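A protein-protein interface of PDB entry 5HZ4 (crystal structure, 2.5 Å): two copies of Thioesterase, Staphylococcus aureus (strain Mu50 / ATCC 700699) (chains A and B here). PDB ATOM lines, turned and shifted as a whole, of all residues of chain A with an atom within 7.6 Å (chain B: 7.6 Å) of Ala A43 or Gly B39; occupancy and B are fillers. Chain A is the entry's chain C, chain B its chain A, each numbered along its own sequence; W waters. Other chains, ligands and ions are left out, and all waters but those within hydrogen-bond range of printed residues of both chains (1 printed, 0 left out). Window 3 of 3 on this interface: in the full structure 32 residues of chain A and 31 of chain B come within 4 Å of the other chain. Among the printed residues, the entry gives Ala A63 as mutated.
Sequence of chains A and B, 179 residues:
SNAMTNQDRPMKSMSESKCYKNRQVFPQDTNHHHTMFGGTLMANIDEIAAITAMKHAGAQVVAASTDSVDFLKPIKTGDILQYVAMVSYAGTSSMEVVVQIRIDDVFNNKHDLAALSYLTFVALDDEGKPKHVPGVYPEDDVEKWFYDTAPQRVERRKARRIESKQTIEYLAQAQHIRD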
ATOM      1  N   LYS A  21      31.548  33.139  -4.387  1.00  0.00           N
ATOM      2  CA  LYS A  21      30.507  33.819  -3.639  1.00  0.00           C
ATOM      3  C   LYS A  21      30.968  35.182  -3.244  1.00  0.00           C
ATOM      4  O   LYS A  21      31.904  35.328  -2.455  1.00  0.00           O
ATOM      5  CB  LYS A  21      30.073  33.018  -2.403  1.00  0.00           C
ATOM      6  CG  LYS A  21      29.121  33.798  -1.545  1.00  0.00           C
ATOM      7  CD  LYS A  21      28.173  32.911  -0.751  1.00  0.00           C
ATOM      8  CE  LYS A  21      28.863  31.990   0.208  1.00  0.00           C
ATOM      9  NZ  LYS A  21      27.827  31.209   0.953  1.00  0.00           N
ATOM     10  N   PHE A  37      31.425  38.552  12.739  1.00  0.00           N
ATOM     11  CA  PHE A  37      31.184  37.365  13.551  1.00  0.00           C
ATOM     12  C   PHE A  37      31.882  36.151  12.896  1.00  0.00           C
ATOM     13  O   PHE A  37      31.742  35.883  11.694  1.00  0.00           O
ATOM     14  CB  PHE A  37      29.654  37.176  13.725  1.00  0.00           C
ATOM     15  CG  PHE A  37      29.238  35.928  14.493  1.00  0.00           C
ATOM     16  CD1 PHE A  37      29.729  35.651  15.772  1.00  0.00           C
ATOM     17  CD2 PHE A  37      28.288  35.053  13.947  1.00  0.00           C
ATOM     18  CE1 PHE A  37      29.305  34.494  16.469  1.00  0.00           C
ATOM     19  CE2 PHE A  37      27.863  33.902  14.635  1.00  0.00           C
ATOM     20  CZ  PHE A  37      28.389  33.616  15.893  1.00  0.00           C
ATOM     21  N   GLY A  38      32.709  35.466  13.673  1.00  0.00           N
ATOM     22  CA  GLY A  38      33.374  34.269  13.191  1.00  0.00           C
ATOM     23  C   GLY A  38      32.404  33.192  12.737  1.00  0.00           C
ATOM     24  O   GLY A  38      32.663  32.462  11.774  1.00  0.00           O
ATOM     25  N   GLY A  39      31.276  33.110  13.432  1.00  0.00           N
ATOM     26  CA  GLY A  39      30.273  32.103  13.146  1.00  0.00           C
ATOM     27  C   GLY A  39      29.650  32.323  11.789  1.00  0.00           C
ATOM     28  O   GLY A  39      29.423  31.365  11.044  1.00  0.00           O
ATOM     29  N   THR A  40      29.408  33.589  11.460  1.00  0.00           N
ATOM     30  CA  THR A  40      28.878  33.972  10.158  1.00  0.00           C
ATOM     31  C   THR A  40      29.841  33.620   9.038  1.00  0.00           C
ATOM     32  O   THR A  40      29.423  33.125   7.996  1.00  0.00           O
ATOM     33  CB  THR A  40      28.564  35.448  10.106  1.00  0.00           C
ATOM     34  OG1 THR A  40      27.656  35.753  11.168  1.00  0.00           O
ATOM     35  CG2 THR A  40      27.922  35.808   8.762  1.00  0.00           C
ATOM     36  N   LEU A  41      31.127  33.906   9.230  1.00  0.00           N
ATOM     37  CA  LEU A  41      32.105  33.499   8.233  1.00  0.00           C
ATOM     38  C   LEU A  41      32.045  31.967   8.055  1.00  0.00           C
ATOM     39  O   LEU A  41      32.018  31.455   6.941  1.00  0.00           O
ATOM     40  CB  LEU A  41      33.509  33.968   8.619  1.00  0.00           C
ATOM     41  CG  LEU A  41      34.603  33.887   7.543  1.00  0.00           C
ATOM     42  CD1 LEU A  41      34.286  34.755   6.345  1.00  0.00           C
ATOM     43  CD2 LEU A  41      35.925  34.310   8.131  1.00  0.00           C
ATOM     44  N   MET A  42      31.978  31.240   9.153  1.00  0.00           N
ATOM     45  CA  MET A  42      31.946  29.785   9.096  1.00  0.00           C
ATOM     46  C   MET A  42      30.664  29.211   8.466  1.00  0.00           C
ATOM     47  O   MET A  42      30.709  28.170   7.837  1.00  0.00           O
ATOM     48  CB  MET A  42      32.152  29.231  10.502  1.00  0.00           C
ATOM     49  CG  MET A  42      33.623  29.172  10.923  1.00  0.00           C
ATOM     50  SD  MET A  42      33.864  28.376  12.540  1.00  0.00           S
ATOM     51  CE  MET A  42      33.465  29.761  13.606  1.00  0.00           C
ATOM     52  N   ALA A  43      29.531  29.885   8.618  1.00  0.00           N
ATOM     53  CA  ALA A  43      28.296  29.394   8.009  1.00  0.00           C
ATOM     54  C   ALA A  43      28.399  29.523   6.483  1.00  0.00           C
ATOM     55  O   ALA A  43      28.102  28.589   5.734  1.00  0.00           O
ATOM     56  CB  ALA A  43      27.079  30.158   8.554  1.00  0.00           C
ATOM     57  N   ASN A  44      28.881  30.668   6.033  1.00  0.00           N
ATOM     58  CA  ASN A  44      29.084  30.901   4.620  1.00  0.00           C
ATOM     59  C   ASN A  44      30.132  29.968   4.029  1.00  0.00           C
ATOM     60  O   ASN A  44      29.956  29.455   2.923  1.00  0.00           O
ATOM     61  CB  ASN A  44      29.490  32.349   4.398  1.00  0.00           C
ATOM     62  CG  ASN A  44      28.339  33.302   4.604  1.00  0.00           C
ATOM     63  OD1 ASN A  44      27.456  33.410   3.764  1.00  0.00           O
ATOM     64  ND2 ASN A  44      28.355  34.016   5.713  1.00  0.00           N
ATOM     65  N   ILE A  45      31.209  29.733   4.783  1.00  0.00           N
ATOM     66  CA  ILE A  45      32.251  28.805   4.370  1.00  0.00           C
ATOM     67  C   ILE A  45      31.615  27.440   4.197  1.00  0.00           C
ATOM     68  O   ILE A  45      31.839  26.750   3.197  1.00  0.00           O
ATOM     69  CB  ILE A  45      33.428  28.709   5.396  1.00  0.00           C
ATOM     70  CG1 ILE A  45      34.317  29.965   5.358  1.00  0.00           C
ATOM     71  CG2 ILE A  45      34.318  27.483   5.121  1.00  0.00           C
ATOM     72  CD1 ILE A  45      35.317  29.989   6.516  1.00  0.00           C
ATOM     73  N   ASP A  46      30.818  27.045   5.185  1.00  0.00           N
ATOM     74  CA  ASP A  46      30.171  25.748   5.124  1.00  0.00           C
ATOM     75  C   ASP A  46      29.238  25.589   3.938  1.00  0.00           C
ATOM     76  O   ASP A  46      29.175  24.527   3.327  1.00  0.00           O
ATOM     77  CB  ASP A  46      29.377  25.494   6.391  1.00  0.00           C
ATOM     78  CG  ASP A  46      28.650  24.181   6.343  1.00  0.00           C
ATOM     79  OD1 ASP A  46      29.339  23.129   6.344  1.00  0.00           O
ATOM     80  OD2 ASP A  46      27.396  24.212   6.272  1.00  0.00           O
ATOM     81  N   GLU A  47      28.504  26.656   3.636  1.00  0.00           N
ATOM     82  CA  GLU A  47      27.546  26.666   2.544  1.00  0.00           C
ATOM     83  C   GLU A  47      28.236  26.533   1.171  1.00  0.00           C
ATOM     84  O   GLU A  47      27.839  25.712   0.354  1.00  0.00           O
ATOM     85  CB  GLU A  47      26.713  27.946   2.615  1.00  0.00           C
ATOM     86  CG  GLU A  47      25.888  28.254   1.385  1.00  0.00           C
ATOM     87  CD  GLU A  47      24.919  29.400   1.609  1.00  0.00           C
ATOM     88  OE1 GLU A  47      25.309  30.399   2.250  1.00  0.00           O
ATOM     89  OE2 GLU A  47      23.772  29.317   1.136  1.00  0.00           O
ATOM     90  N   ILE A  48      29.261  27.350   0.921  1.00  0.00           N
ATOM     91  CA  ILE A  48      29.968  27.342  -0.362  1.00  0.00           C
ATOM     92  C   ILE A  48      30.735  26.026  -0.537  1.00  0.00           C
ATOM     93  O   ILE A  48      30.805  25.486  -1.629  1.00  0.00           O
ATOM     94  CB  ILE A  48      30.949  28.579  -0.495  1.00  0.00           C
ATOM     95  CG1 ILE A  48      31.451  28.768  -1.928  1.00  0.00           C
ATOM     96  CG2 ILE A  48      32.149  28.487   0.435  1.00  0.00           C
ATOM     97  CD1 ILE A  48      30.362  29.042  -2.924  1.00  0.00           C
ATOM     98  N   ALA A  49      31.318  25.508   0.538  1.00  0.00           N
ATOM     99  CA  ALA A  49      32.110  24.288   0.440  1.00  0.00           C
ATOM    100  C   ALA A  49      31.237  23.060   0.124  1.00  0.00           C
ATOM    101  O   ALA A  49      31.656  22.184  -0.639  1.00  0.00           O
ATOM    102  CB  ALA A  49      32.911  24.064   1.735  1.00  0.00           C
ATOM    103  N   ALA A  63      29.207  16.728   5.543  1.00  0.00           N
ATOM    104  CA  ALA A  63      30.360  17.261   6.241  1.00  0.00           C
ATOM    105  C   ALA A  63      30.850  16.216   7.266  1.00  0.00           C
ATOM    106  O   ALA A  63      30.111  15.857   8.187  1.00  0.00           O
ATOM    107  CB  ALA A  63      30.025  18.581   6.923  1.00  0.00           C
ATOM    108  N   THR A  66      35.110  20.078   9.886  1.00  0.00           N
ATOM    109  CA  THR A  66      35.801  21.322   9.584  1.00  0.00           C
ATOM    110  C   THR A  66      37.180  21.197  10.193  1.00  0.00           C
ATOM    111  O   THR A  66      37.329  21.156  11.427  1.00  0.00           O
ATOM    112  CB  THR A  66      35.099  22.535  10.144  1.00  0.00           C
ATOM    113  OG1 THR A  66      33.873  22.740   9.451  1.00  0.00           O
ATOM    114  CG2 THR A  66      35.986  23.789   9.990  1.00  0.00           C
ATOM    115  N   TYR A  83      34.400  34.587  -1.530  1.00  0.00           N
ATOM    116  CA  TYR A  83      34.702  33.226  -1.121  1.00  0.00           C
ATOM    117  C   TYR A  83      35.057  32.417  -2.338  1.00  0.00           C
ATOM    118  O   TYR A  83      34.323  32.440  -3.329  1.00  0.00           O
ATOM    119  CB  TYR A  83      33.509  32.566  -0.433  1.00  0.00           C
ATOM    120  CG  TYR A  83      33.015  33.258   0.808  1.00  0.00           C
ATOM    121  CD1 TYR A  83      32.225  34.400   0.732  1.00  0.00           C
ATOM    122  CD2 TYR A  83      33.314  32.752   2.059  1.00  0.00           C
ATOM    123  CE1 TYR A  83      31.762  35.021   1.865  1.00  0.00           C
ATOM    124  CE2 TYR A  83      32.858  33.366   3.197  1.00  0.00           C
ATOM    125  CZ  TYR A  83      32.087  34.497   3.100  1.00  0.00           C
ATOM    126  OH  TYR A  83      31.626  35.078   4.252  1.00  0.00           O
ATOM    127  N   ASP B  29      16.796  25.383  10.537  1.00  0.00           N
ATOM    128  CA  ASP B  29      18.153  25.096  10.965  1.00  0.00           C
ATOM    129  C   ASP B  29      18.702  23.871  10.219  1.00  0.00           C
ATOM    130  O   ASP B  29      19.918  23.633  10.218  1.00  0.00           O
ATOM    131  CB  ASP B  29      18.207  24.826  12.475  1.00  0.00           C
ATOM    132  CG  ASP B  29      17.962  26.061  13.316  1.00  0.00           C
ATOM    133  OD1 ASP B  29      18.051  27.180  12.759  1.00  0.00           O
ATOM    134  OD2 ASP B  29      17.704  25.898  14.544  1.00  0.00           O
ATOM    135  N   MET B  36      20.940  18.886  10.492  1.00  0.00           N
ATOM    136  CA  MET B  36      21.328  20.253  10.846  1.00  0.00           C
ATOM    137  C   MET B  36      22.432  20.831   9.939  1.00  0.00           C
ATOM    138  O   MET B  36      23.388  20.148   9.563  1.00  0.00           O
ATOM    139  CB  MET B  36      21.787  20.348  12.304  1.00  0.00           C
ATOM    140  CG  MET B  36      21.961  21.791  12.782  1.00  0.00           C
ATOM    141  SD  MET B  36      22.399  22.058  14.531  1.00  0.00           S
ATOM    142  CE  MET B  36      21.263  23.371  14.987  1.00  0.00           C
ATOM    143  N   PHE B  37      22.251  22.084   9.542  1.00  0.00           N
ATOM    144  CA  PHE B  37      23.264  22.792   8.788  1.00  0.00           C
ATOM    145  C   PHE B  37      24.553  22.842   9.590  1.00  0.00           C
ATOM    146  O   PHE B  37      24.543  23.183  10.776  1.00  0.00           O
ATOM    147  CB  PHE B  37      22.780  24.204   8.461  1.00  0.00           C
ATOM    148  CG  PHE B  37      21.800  24.252   7.321  1.00  0.00           C
ATOM    149  CD1 PHE B  37      21.921  23.363   6.253  1.00  0.00           C
ATOM    150  CD2 PHE B  37      20.717  25.135   7.352  1.00  0.00           C
ATOM    151  CE1 PHE B  37      21.017  23.397   5.215  1.00  0.00           C
ATOM    152  CE2 PHE B  37      19.800  25.165   6.318  1.00  0.00           C
ATOM    153  CZ  PHE B  37      19.948  24.301   5.251  1.00  0.00           C
ATOM    154  N   GLY B  38      25.650  22.423   8.973  1.00  0.00           N
ATOM    155  CA  GLY B  38      26.948  22.520   9.607  1.00  0.00           C
ATOM    156  C   GLY B  38      27.270  23.966   9.971  1.00  0.00           C
ATOM    157  O   GLY B  38      27.923  24.242  10.987  1.00  0.00           O
ATOM    158  N   GLY B  39      26.811  24.892   9.136  1.00  0.00           N
ATOM    159  CA  GLY B  39      27.082  26.297   9.330  1.00  0.00           C
ATOM    160  C   GLY B  39      26.391  26.834  10.557  1.00  0.00           C
ATOM    161  O   GLY B  39      26.959  27.644  11.286  1.00  0.00           O
ATOM    162  N   THR B  40      25.158  26.395  10.770  1.00  0.00           N
ATOM    163  CA  THR B  40      24.409  26.776  11.957  1.00  0.00           C
ATOM    164  C   THR B  40      25.054  26.230  13.226  1.00  0.00           C
ATOM    165  O   THR B  40      25.139  26.942  14.226  1.00  0.00           O
ATOM    166  CB  THR B  40      22.954  26.323  11.871  1.00  0.00           C
ATOM    167  OG1 THR B  40      22.364  26.905  10.707  1.00  0.00           O
ATOM    168  CG2 THR B  40      22.159  26.792  13.091  1.00  0.00           C
ATOM    169  N   LEU B  41      25.466  24.966  13.214  1.00  0.00           N
ATOM    170  CA  LEU B  41      26.152  24.428  14.390  1.00  0.00           C
ATOM    171  C   LEU B  41      27.416  25.251  14.699  1.00  0.00           C
ATOM    172  O   LEU B  41      27.678  25.602  15.856  1.00  0.00           O
ATOM    173  CB  LEU B  41      26.526  22.946  14.219  1.00  0.00           C
ATOM    174  CG  LEU B  41      26.937  22.298  15.555  1.00  0.00           C
ATOM    175  CD1 LEU B  41      25.777  22.279  16.539  1.00  0.00           C
ATOM    176  CD2 LEU B  41      27.529  20.906  15.403  1.00  0.00           C
ATOM    177  N   MET B  42      28.180  25.573  13.661  1.00  0.00           N
ATOM    178  CA  MET B  42      29.429  26.295  13.847  1.00  0.00           C
ATOM    179  C   MET B  42      29.212  27.723  14.359  1.00  0.00           C
ATOM    180  O   MET B  42      29.993  28.210  15.150  1.00  0.00           O
ATOM    181  CB  MET B  42      30.232  26.305  12.545  1.00  0.00           C
ATOM    182  CG  MET B  42      31.011  25.019  12.302  1.00  0.00           C
ATOM    183  SD  MET B  42      32.134  25.076  10.880  1.00  0.00           S
ATOM    184  CE  MET B  42      30.972  24.838   9.524  1.00  0.00           C
ATOM    185  N   ALA B  43      28.122  28.371  13.974  1.00  0.00           N
ATOM    186  CA  ALA B  43      27.875  29.729  14.449  1.00  0.00           C
ATOM    187  C   ALA B  43      27.590  29.739  15.959  1.00  0.00           C
ATOM    188  O   ALA B  43      28.109  30.564  16.704  1.00  0.00           O
ATOM    189  CB  ALA B  43      26.714  30.358  13.668  1.00  0.00           C
ATOM    190  N   ASN B  44      26.771  28.792  16.391  1.00  0.00           N
ATOM    191  CA  ASN B  44      26.431  28.627  17.780  1.00  0.00           C
ATOM    192  C   ASN B  44      27.672  28.270  18.599  1.00  0.00           C
ATOM    193  O   ASN B  44      27.842  28.732  19.743  1.00  0.00           O
ATOM    194  CB  ASN B  44      25.371  27.534  17.933  1.00  0.00           C
ATOM    195  CG  ASN B  44      24.003  27.956  17.394  1.00  0.00           C
ATOM    196  OD1 ASN B  44      23.299  28.752  17.998  1.00  0.00           O
ATOM    197  ND2 ASN B  44      23.607  27.370  16.279  1.00  0.00           N
ATOM    198  N   ILE B  45      28.527  27.430  18.015  1.00  0.00           N
ATOM    199  CA  ILE B  45      29.779  27.042  18.642  1.00  0.00           C
ATOM    200  C   ILE B  45      30.613  28.273  18.858  1.00  0.00           C
ATOM    201  O   ILE B  45      31.153  28.482  19.940  1.00  0.00           O
ATOM    202  CB  ILE B  45      30.571  26.003  17.806  1.00  0.00           C
ATOM    203  CG1 ILE B  45      29.920  24.617  17.942  1.00  0.00           C
ATOM    204  CG2 ILE B  45      32.033  25.915  18.271  1.00  0.00           C
ATOM    205  CD1 ILE B  45      30.447  23.587  16.974  1.00  0.00           C
ATOM    206  N   PHE B  71      32.214  16.360  13.276  1.00  0.00           N
ATOM    207  CA  PHE B  71      30.806  15.936  13.263  1.00  0.00           C
ATOM    208  C   PHE B  71      30.737  14.426  13.450  1.00  0.00           C
ATOM    209  O   PHE B  71      31.197  13.661  12.595  1.00  0.00           O
ATOM    210  CB  PHE B  71      30.111  16.372  11.970  1.00  0.00           C
ATOM    211  CG  PHE B  71      30.122  17.870  11.763  1.00  0.00           C
ATOM    212  CD1 PHE B  71      30.994  18.466  10.865  1.00  0.00           C
ATOM    213  CD2 PHE B  71      29.287  18.688  12.489  1.00  0.00           C
ATOM    214  CE1 PHE B  71      31.000  19.843  10.680  1.00  0.00           C
ATOM    215  CE2 PHE B  71      29.306  20.070  12.295  1.00  0.00           C
ATOM    216  CZ  PHE B  71      30.151  20.634  11.391  1.00  0.00           C
HETATM  217  O   HOH W   1      25.636  22.173   5.826  1.00  0.00           O
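Ala B43 touches Phe A37 (O to CZ, 3.2 Å).
Ala B43 touches Gly A39 (CA to CA, 3.6 Å).
Met A42 touches Met B42 (O to CE, 3.7 Å).
Gly B39 touches Ala A43 (CA to CA, 3.6 Å).
Asp A46 touches Gly B38.
CE of Met B42 touches CB of Asp A46 (3.6 Å).
Ala A63 touches Phe B71.
Phe A37 touches Ala B43, but with the chains exchanged Ala A43 does not touch Phe B37 (7.3 Å).
Gly A39 touches Ala B43, and with the chains exchanged Ala A43 touches Gly B39.
Met A42 touches its own counterpart, Met B42.
Positions printed for both chains: 37, 38, 39, 40, 41, 42, 43, 44 and 45.
Water W1 lies within hydrogen-bond range of OD2 of Asp A46 (2.7 Å) and N of Gly B38 (3.2 Å).
SD of Met B42 sits at hydrogen-bond distance from OG1 of Thr A66.
The backbone NH (N) of Gly B39 sits at hydrogen-bond distance from the side-chain carboxylate (OD2) of Asp A46.
Hydrophobic or aromatic side chains of chain A that line the printed part of chain B: Phe A37 and Ala A43.
Printed residues of chain B that touch a printed residue of chain A: Gly B38, Gly B39, Met B42, Ala B43 and Phe B71.
Among the printed residues, 9 pairs touch across the chains.
Of the printed residues of chain B, Phe A37 touches Ala B43 (3.2 Å).
Of the printed residues of chain B, Met A42 touches Met B42.
Ala A43 touches one residue of chain B.
Of chain A, only Ala A43 (3.6 Å) and Asp A46 (3.0 Å) come within 4 Å of Gly B39.
Printed residues of chain A within 4 Å of Phe B71: Ala A63 (3.8 Å).
The nearest residue of chain B that does not touch Ala A43 is Thr B40 (4.8 Å).
The nearest residue of chain A that does not touch Gly B39 is Met A42 (4.3 Å).
The nearest printed residue of chain A that does not touch Phe B71 is Thr A66 (4.2 Å).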
